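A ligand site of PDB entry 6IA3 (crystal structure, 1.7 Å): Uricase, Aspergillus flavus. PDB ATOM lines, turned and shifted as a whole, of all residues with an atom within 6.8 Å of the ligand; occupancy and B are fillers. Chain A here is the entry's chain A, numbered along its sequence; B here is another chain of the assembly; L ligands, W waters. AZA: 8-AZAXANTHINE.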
ATOM      1  N   SER A 158     -27.675   1.586  23.698  1.00  0.00           N
ATOM      2  CA  SER A 158     -27.338   2.887  23.120  1.00  0.00           C
ATOM      3  C   SER A 158     -28.584   3.750  23.201  1.00  0.00           C
ATOM      4  O   SER A 158     -29.660   3.223  22.942  1.00  0.00           O
ATOM      5  CB  SER A 158     -26.792   2.765  21.709  1.00  0.00           C
ATOM      6  OG  SER A 158     -26.631   4.068  21.132  1.00  0.00           O
ATOM      7  N   GLN A 159     -28.411   5.000  23.623  1.00  0.00           N
ATOM      8  CA  GLN A 159     -29.473   5.993  23.833  1.00  0.00           C
ATOM      9  C   GLN A 159     -29.071   7.298  23.160  1.00  0.00           C
ATOM     10  O   GLN A 159     -27.877   7.599  22.989  1.00  0.00           O
ATOM     11  CB  GLN A 159     -29.726   6.195  25.319  1.00  0.00           C
ATOM     12  CG  GLN A 159     -29.888   4.870  26.059  1.00  0.00           C
ATOM     13  CD  GLN A 159     -30.290   5.087  27.489  1.00  0.00           C
ATOM     14  OE1 GLN A 159     -31.090   5.961  27.811  1.00  0.00           O
ATOM     15  NE2 GLN A 159     -29.796   4.221  28.362  1.00  0.00           N
ATOM     16  N   PHE A 160     -30.059   8.122  22.837  1.00  0.00           N
ATOM     17  CA  PHE A 160     -29.780   9.504  22.397  1.00  0.00           C
ATOM     18  C   PHE A 160     -31.009  10.362  22.677  1.00  0.00           C
ATOM     19  O   PHE A 160     -31.999  10.302  21.930  1.00  0.00           O
ATOM     20  CB  PHE A 160     -29.318   9.569  20.941  1.00  0.00           C
ATOM     21  CG  PHE A 160     -28.712  10.911  20.642  1.00  0.00           C
ATOM     22  CD1 PHE A 160     -27.646  11.388  21.390  1.00  0.00           C
ATOM     23  CD2 PHE A 160     -29.240  11.745  19.670  1.00  0.00           C
ATOM     24  CE1 PHE A 160     -27.077  12.616  21.109  1.00  0.00           C
ATOM     25  CE2 PHE A 160     -28.677  12.983  19.397  1.00  0.00           C
ATOM     26  CZ  PHE A 160     -27.618  13.439  20.143  1.00  0.00           C
ATOM     27  N   PHE A 163     -31.069  16.160  23.503  1.00  0.00           N
ATOM     28  CA  PHE A 163     -30.394  17.066  22.536  1.00  0.00           C
ATOM     29  C   PHE A 163     -31.262  18.285  22.229  1.00  0.00           C
ATOM     30  O   PHE A 163     -32.479  18.318  22.555  1.00  0.00           O
ATOM     31  CB  PHE A 163     -30.005  16.341  21.256  1.00  0.00           C
ATOM     32  CG  PHE A 163     -31.118  15.550  20.623  1.00  0.00           C
ATOM     33  CD1 PHE A 163     -31.972  16.149  19.702  1.00  0.00           C
ATOM     34  CD2 PHE A 163     -31.328  14.230  20.961  1.00  0.00           C
ATOM     35  CE1 PHE A 163     -33.007  15.426  19.138  1.00  0.00           C
ATOM     36  CE2 PHE A 163     -32.366  13.494  20.401  1.00  0.00           C
ATOM     37  CZ  PHE A 163     -33.211  14.108  19.490  1.00  0.00           C
ATOM     38  N   LEU A 171     -35.678  14.732  14.702  1.00  0.00           N
ATOM     39  CA  LEU A 171     -35.198  13.475  15.304  1.00  0.00           C
ATOM     40  C   LEU A 171     -35.962  13.177  16.603  1.00  0.00           C
ATOM     41  O   LEU A 171     -36.013  14.057  17.483  1.00  0.00           O
ATOM     42  CB  LEU A 171     -33.703  13.614  15.593  1.00  0.00           C
ATOM     43  CG  LEU A 171     -33.071  12.359  16.187  1.00  0.00           C
ATOM     44  CD1 LEU A 171     -33.176  11.185  15.234  1.00  0.00           C
ATOM     45  CD2 LEU A 171     -31.622  12.638  16.542  1.00  0.00           C
ATOM     46  N   ARG A 177     -31.475   2.169  20.946  1.00  0.00           N
ATOM     47  CA  ARG A 177     -31.178   2.185  19.499  1.00  0.00           C
ATOM     48  C   ARG A 177     -29.975   1.310  19.223  1.00  0.00           C
ATOM     49  O   ARG A 177     -29.334   0.828  20.165  1.00  0.00           O
ATOM     50  CB  ARG A 177     -30.922   3.623  19.017  1.00  0.00           C
ATOM     51  CG  ARG A 177     -29.625   4.241  19.563  1.00  0.00           C
ATOM     52  CD  ARG A 177     -29.350   5.634  19.016  1.00  0.00           C
ATOM     53  NE  ARG A 177     -28.060   6.087  19.495  1.00  0.00           N
ATOM     54  CZ  ARG A 177     -27.416   7.176  19.104  1.00  0.00           C
ATOM     55  NH1 ARG A 177     -27.953   8.014  18.227  1.00  0.00           N
ATOM     56  NH2 ARG A 177     -26.204   7.420  19.595  1.00  0.00           N
ATOM     57  N   LEU A 179     -26.197   1.070  17.741  1.00  0.00           N
ATOM     58  CA  LEU A 179     -24.998   1.919  17.518  1.00  0.00           C
ATOM     59  C   LEU A 179     -23.967   1.087  16.772  1.00  0.00           C
ATOM     60  O   LEU A 179     -23.612  -0.009  17.210  1.00  0.00           O
ATOM     61  CB  LEU A 179     -24.454   2.439  18.851  1.00  0.00           C
ATOM     62  CG  LEU A 179     -23.172   3.261  18.751  1.00  0.00           C
ATOM     63  CD1 LEU A 179     -23.343   4.506  17.890  1.00  0.00           C
ATOM     64  CD2 LEU A 179     -22.682   3.628  20.149  1.00  0.00           C
ATOM     65  N   SER A 225     -24.633   3.655  26.399  1.00  0.00           N
ATOM     66  CA  SER A 225     -24.086   4.883  25.760  1.00  0.00           C
ATOM     67  C   SER A 225     -25.134   6.011  25.753  1.00  0.00           C
ATOM     68  O   SER A 225     -26.236   5.809  25.231  1.00  0.00           O
ATOM     69  CB  SER A 225     -23.633   4.571  24.364  1.00  0.00           C
ATOM     70  OG  SER A 225     -23.217   5.763  23.726  1.00  0.00           O
ATOM     71  N   ALA A 226     -24.742   7.192  26.194  1.00  0.00           N
ATOM     72  CA  ALA A 226     -25.584   8.407  26.228  1.00  0.00           C
ATOM     73  C   ALA A 226     -25.480   9.123  24.879  1.00  0.00           C
ATOM     74  O   ALA A 226     -26.351   9.940  24.548  1.00  0.00           O
ATOM     75  CB  ALA A 226     -25.131   9.307  27.350  1.00  0.00           C
ATOM     76  N   SER A 227     -24.415   8.822  24.141  1.00  0.00           N
ATOM     77  CA  SER A 227     -24.079   9.442  22.838  1.00  0.00           C
ATOM     78  C   SER A 227     -22.765   8.831  22.357  1.00  0.00           C
ATOM     79  O   SER A 227     -22.034   8.271  23.186  1.00  0.00           O
ATOM     80  CB  SER A 227     -23.945  10.951  22.894  1.00  0.00           C
ATOM     81  OG  SER A 227     -22.845  11.319  23.731  1.00  0.00           O
ATOM     82  N   VAL A 228     -22.449   8.991  21.088  1.00  0.00           N
ATOM     83  CA  VAL A 228     -21.095   8.637  20.576  1.00  0.00           C
ATOM     84  C   VAL A 228     -20.059   9.478  21.350  1.00  0.00           C
ATOM     85  O   VAL A 228     -19.020   8.890  21.777  1.00  0.00           O
ATOM     86  CB  VAL A 228     -21.006   8.839  19.050  1.00  0.00           C
ATOM     87  CG1 VAL A 228     -19.602   8.545  18.566  1.00  0.00           C
ATOM     88  CG2 VAL A 228     -21.997   7.938  18.325  1.00  0.00           C
ATOM     89  N   GLN A 229     -20.325  10.770  21.507  1.00  0.00           N
ATOM     90  CA  GLN A 229     -19.454  11.739  22.213  1.00  0.00           C
ATOM     91  C   GLN A 229     -19.058  11.128  23.576  1.00  0.00           C
ATOM     92  O   GLN A 229     -17.846  11.086  23.901  1.00  0.00           O
ATOM     93  CB  GLN A 229     -20.184  13.075  22.367  1.00  0.00           C
ATOM     94  CG  GLN A 229     -20.315  13.873  21.066  1.00  0.00           C
ATOM     95  CD  GLN A 229     -21.549  13.596  20.244  1.00  0.00           C
ATOM     96  OE1 GLN A 229     -22.108  12.500  20.242  1.00  0.00           O
ATOM     97  NE2 GLN A 229     -21.952  14.590  19.459  1.00  0.00           N
ATOM     98  N   ASN A 255     -21.318   7.683  12.843  1.00  0.00           N
ATOM     99  CA  ASN A 255     -22.538   7.067  13.397  1.00  0.00           C
ATOM    100  C   ASN A 255     -23.266   6.419  12.232  1.00  0.00           C
ATOM    101  O   ASN A 255     -23.817   7.168  11.414  1.00  0.00           O
ATOM    102  CB  ASN A 255     -23.386   8.091  14.129  1.00  0.00           C
ATOM    103  CG  ASN A 255     -24.465   7.477  15.001  1.00  0.00           C
ATOM    104  OD1 ASN A 255     -24.603   6.262  15.065  1.00  0.00           O
ATOM    105  ND2 ASN A 255     -25.191   8.327  15.693  1.00  0.00           N
ATOM    106  N   HIS A 257     -25.978   4.823  10.739  1.00  0.00           N
ATOM    107  CA  HIS A 257     -27.376   4.786  11.228  1.00  0.00           C
ATOM    108  C   HIS A 257     -28.064   3.515  10.744  1.00  0.00           C
ATOM    109  O   HIS A 257     -27.902   3.144   9.561  1.00  0.00           O
ATOM    110  CB  HIS A 257     -28.120   6.034  10.785  1.00  0.00           C
ATOM    111  CG  HIS A 257     -27.431   7.291  11.193  1.00  0.00           C
ATOM    112  ND1 HIS A 257     -27.273   7.661  12.525  1.00  0.00           N
ATOM    113  CD2 HIS A 257     -26.860   8.251  10.439  1.00  0.00           C
ATOM    114  CE1 HIS A 257     -26.656   8.832  12.565  1.00  0.00           C
ATOM    115  NE2 HIS A 257     -26.359   9.215  11.283  1.00  0.00           N
ATOM    116  N   GLY A 287     -23.654  10.533  10.735  1.00  0.00           N
ATOM    117  CA  GLY A 287     -23.016  11.333  11.777  1.00  0.00           C
ATOM    118  C   GLY A 287     -21.515  11.111  11.737  1.00  0.00           C
ATOM    119  O   GLY A 287     -21.062   9.992  11.383  1.00  0.00           O
ATOM    120  N   ILE A 289     -18.317  12.131  14.363  1.00  0.00           N
ATOM    121  CA  ILE A 289     -18.022  12.637  15.720  1.00  0.00           C
ATOM    122  C   ILE A 289     -16.520  12.523  15.959  1.00  0.00           C
ATOM    123  O   ILE A 289     -15.979  11.424  15.828  1.00  0.00           O
ATOM    124  CB  ILE A 289     -18.824  11.833  16.773  1.00  0.00           C
ATOM    125  CG1 ILE A 289     -20.265  11.507  16.327  1.00  0.00           C
ATOM    126  CG2 ILE A 289     -18.768  12.548  18.099  1.00  0.00           C
ATOM    127  CD1 ILE A 289     -21.166  12.671  16.122  1.00  0.00           C
ATOM    128  N   TYR B   9     -18.076  17.854  15.434  1.00  0.00           N
ATOM    129  CA  TYR B   9     -19.037  16.762  15.119  1.00  0.00           C
ATOM    130  C   TYR B   9     -20.051  17.348  14.133  1.00  0.00           C
ATOM    131  O   TYR B   9     -20.298  18.566  14.099  1.00  0.00           O
ATOM    132  CB  TYR B   9     -19.688  16.222  16.402  1.00  0.00           C
ATOM    133  CG  TYR B   9     -20.868  17.068  16.794  1.00  0.00           C
ATOM    134  CD1 TYR B   9     -20.679  18.343  17.300  1.00  0.00           C
ATOM    135  CD2 TYR B   9     -22.146  16.699  16.433  1.00  0.00           C
ATOM    136  CE1 TYR B   9     -21.746  19.204  17.508  1.00  0.00           C
ATOM    137  CE2 TYR B   9     -23.216  17.562  16.603  1.00  0.00           C
ATOM    138  CZ  TYR B   9     -23.010  18.823  17.134  1.00  0.00           C
ATOM    139  OH  TYR B   9     -24.068  19.671  17.317  1.00  0.00           O
ATOM    140  N   GLY B  10     -20.738  16.468  13.407  1.00  0.00           N
ATOM    141  CA  GLY B  10     -21.839  16.867  12.541  1.00  0.00           C
ATOM    142  C   GLY B  10     -22.172  15.763  11.574  1.00  0.00           C
ATOM    143  O   GLY B  10     -22.118  14.593  11.970  1.00  0.00           O
ATOM    144  N   LYS B  11     -22.621  16.141  10.367  1.00  0.00           N
ATOM    145  CA  LYS B  11     -23.131  15.143   9.406  1.00  0.00           C
ATOM    146  C   LYS B  11     -22.221  15.158   8.182  1.00  0.00           C
ATOM    147  O   LYS B  11     -21.973  16.258   7.612  1.00  0.00           O
ATOM    148  CB  LYS B  11     -24.593  15.366   9.042  1.00  0.00           C
ATOM    149  CG  LYS B  11     -25.214  14.162   8.358  1.00  0.00           C
ATOM    150  CD  LYS B  11     -25.504  12.996   9.256  1.00  0.00           C
ATOM    151  CE  LYS B  11     -26.902  13.053   9.820  1.00  0.00           C
ATOM    152  NZ  LYS B  11     -27.046  12.184  11.000  1.00  0.00           N
ATOM    153  N   ASN B  52     -26.278  16.262  26.549  1.00  0.00           N
ATOM    154  CA  ASN B  52     -26.720  16.352  25.136  1.00  0.00           C
ATOM    155  C   ASN B  52     -27.376  17.711  24.847  1.00  0.00           C
ATOM    156  O   ASN B  52     -27.602  17.992  23.660  1.00  0.00           O
ATOM    157  CB  ASN B  52     -27.577  15.156  24.735  1.00  0.00           C
ATOM    158  CG  ASN B  52     -26.778  13.880  24.632  1.00  0.00           C
ATOM    159  OD1 ASN B  52     -25.579  13.917  24.352  1.00  0.00           O
ATOM    160  ND2 ASN B  52     -27.426  12.757  24.829  1.00  0.00           N
ATOM    161  N   ILE B  55     -25.842  19.676  22.095  1.00  0.00           N
ATOM    162  CA  ILE B  55     -25.762  19.031  20.755  1.00  0.00           C
ATOM    163  C   ILE B  55     -26.925  19.501  19.876  1.00  0.00           C
ATOM    164  O   ILE B  55     -28.082  19.205  20.200  1.00  0.00           O
ATOM    165  CB  ILE B  55     -25.692  17.503  20.848  1.00  0.00           C
ATOM    166  CG1 ILE B  55     -24.479  17.043  21.676  1.00  0.00           C
ATOM    167  CG2 ILE B  55     -25.632  16.940  19.448  1.00  0.00           C
ATOM    168  CD1 ILE B  55     -24.345  15.551  21.764  1.00  0.00           C
ATOM    169  N   VAL B  56     -26.591  20.199  18.803  1.00  0.00           N
ATOM    170  CA  VAL B  56     -27.457  20.341  17.607  1.00  0.00           C
ATOM    171  C   VAL B  56     -27.365  18.993  16.875  1.00  0.00           C
ATOM    172  O   VAL B  56     -26.229  18.632  16.465  1.00  0.00           O
ATOM    173  CB  VAL B  56     -27.013  21.525  16.753  1.00  0.00           C
ATOM    174  CG1 VAL B  56     -27.835  21.620  15.475  1.00  0.00           C
ATOM    175  CG2 VAL B  56     -27.023  22.840  17.525  1.00  0.00           C
ATOM    176  N   ALA B  57     -28.412  18.181  16.912  1.00  0.00           N
ATOM    177  CA  ALA B  57     -28.337  16.793  16.434  1.00  0.00           C
ATOM    178  C   ALA B  57     -27.759  16.758  15.010  1.00  0.00           C
ATOM    179  O   ALA B  57     -28.113  17.654  14.192  1.00  0.00           O
ATOM    180  CB  ALA B  57     -29.686  16.115  16.479  1.00  0.00           C
ATOM    181  N   THR B  58     -26.915  15.764  14.688  1.00  0.00           N
ATOM    182  CA  THR B  58     -26.406  15.627  13.308  1.00  0.00           C
ATOM    183  C   THR B  58     -27.606  15.519  12.359  1.00  0.00           C
ATOM    184  O   THR B  58     -27.554  16.090  11.249  1.00  0.00           O
ATOM    185  CB  THR B  58     -25.403  14.465  13.191  1.00  0.00           C
ATOM    186  OG1 THR B  58     -26.086  13.226  13.351  1.00  0.00           O
ATOM    187  CG2 THR B  58     -24.286  14.588  14.202  1.00  0.00           C
ATOM    188  N   ASP B  59     -28.670  14.838  12.787  1.00  0.00           N
ATOM    189  CA  ASP B  59     -29.905  14.710  11.968  1.00  0.00           C
ATOM    190  C   ASP B  59     -30.450  16.111  11.646  1.00  0.00           C
ATOM    191  O   ASP B  59     -30.923  16.290  10.528  1.00  0.00           O
ATOM    192  CB  ASP B  59     -30.959  13.880  12.688  1.00  0.00           C
ATOM    193  CG  ASP B  59     -32.135  13.530  11.812  1.00  0.00           C
ATOM    194  OD1 ASP B  59     -32.000  12.572  11.012  1.00  0.00           O
ATOM    195  OD2 ASP B  59     -33.165  14.258  11.895  1.00  0.00           O
ATOM    196  N   SER B  60     -30.454  17.034  12.618  1.00  0.00           N
ATOM    197  CA  SER B  60     -30.889  18.457  12.427  1.00  0.00           C
ATOM    198  C   SER B  60     -29.940  19.204  11.488  1.00  0.00           C
ATOM    199  O   SER B  60     -30.416  20.029  10.695  1.00  0.00           O
ATOM    200  CB  SER B  60     -31.032  19.178  13.747  1.00  0.00           C
ATOM    201  OG  SER B  60     -31.858  18.424  14.637  1.00  0.00           O
HETATM  202  N1  AZA L   1     -24.527  11.938  18.649  1.00  0.00           N
HETATM  203  C2  AZA L   1     -25.113  10.686  18.695  1.00  0.00           C
HETATM  204  O2  AZA L   1     -24.648   9.788  19.392  1.00  0.00           O
HETATM  205  N3  AZA L   1     -26.250  10.485  17.957  1.00  0.00           N
HETATM  206  C4  AZA L   1     -26.782  11.501  17.222  1.00  0.00           C
HETATM  207  C5  AZA L   1     -26.209  12.753  17.204  1.00  0.00           C
HETATM  208  C6  AZA L   1     -25.025  13.033  17.946  1.00  0.00           C
HETATM  209  O6  AZA L   1     -24.398  14.098  17.977  1.00  0.00           O
HETATM  210  N7  AZA L   1     -26.990  13.563  16.403  1.00  0.00           N
HETATM  211  N8  AZA L   1     -27.960  12.834  15.929  1.00  0.00           N
HETATM  212  N9  AZA L   1     -27.875  11.597  16.433  1.00  0.00           N
HETATM  213  O   HOH W   1     -29.381   9.400  15.593  1.00  0.00           O
HETATM  214  O   HOH W   2     -24.703  11.165  14.689  1.00  0.00           O
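OG1 of Thr 58 of chain B sits at hydrogen-bond distance from NZ of Lys 11 of chain B (2.7 Å). The backbone NH (N) of Arg 177 lies within hydrogen-bond range of the backbone carbonyl oxygen (O) of Ser 158, 2.9 Å away. N of Gln 229 sits close to OG of Ser 227, at 3.4 Å. O of Asn 255 lies within hydrogen-bond range of NE2 of His 257 (3.3 Å). N of Asn 255 sits at hydrogen-bond distance from O of Gly 287, at 2.7 Å. O of Ser 227 sits at hydrogen-bond distance from OG of Ser 225. OH of Tyr 9 of chain B sits at hydrogen-bond distance from O of Val 56 of chain B (2.5 Å).
N of Thr 58 of chain B sits at hydrogen-bond distance from N7 of the ligand, 2.8 Å away. The side-chain hydroxyl (OG1) of Thr 58 of chain B is in hydrogen-bond range of a nitrogen (N7) of the ligand. The guanidinium group (NH2) of Arg 177 lies within hydrogen-bond range of an oxygen (O2) of the ligand. N of Val 228 lies within hydrogen-bond range of O2 of the ligand (2.9 Å). The side-chain amide nitrogen (NE2) of Gln 229 lies within hydrogen-bond range of an oxygen (O6) of the ligand, 2.9 Å away. ND2 of Asn 255 lies close to N3 of the ligand, 3.3 Å away.
Merely in contact with the ligand: Phe 160, Leu 171, Ser 227, Ile 289, Tyr 9 of chain B, Ile 55 of chain B, Ala 57 of chain B and Asp 59 of chain B. Hydrophobic or aromatic side chains within 4 Å of the ligand: Phe 160, Leu 171, Val 228, Ile 289, Tyr 9 of chain B, Ile 55 of chain B and Ala 57 of chain B. Along chain A the residues within 4 Å of the ligand span positions 160 to 289.
Water W1 bridges a nitrogen (N9) of the ligand (2.8 Å) and the guanidinium group of Arg 177 (3.3 Å). Water W2 lies within hydrogen-bond range of the side-chain hydroxyl (OG1) of Thr 58 of chain B (2.8 Å) and the side-chain amide nitrogen (ND2) of Asn 255 (3.0 Å).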
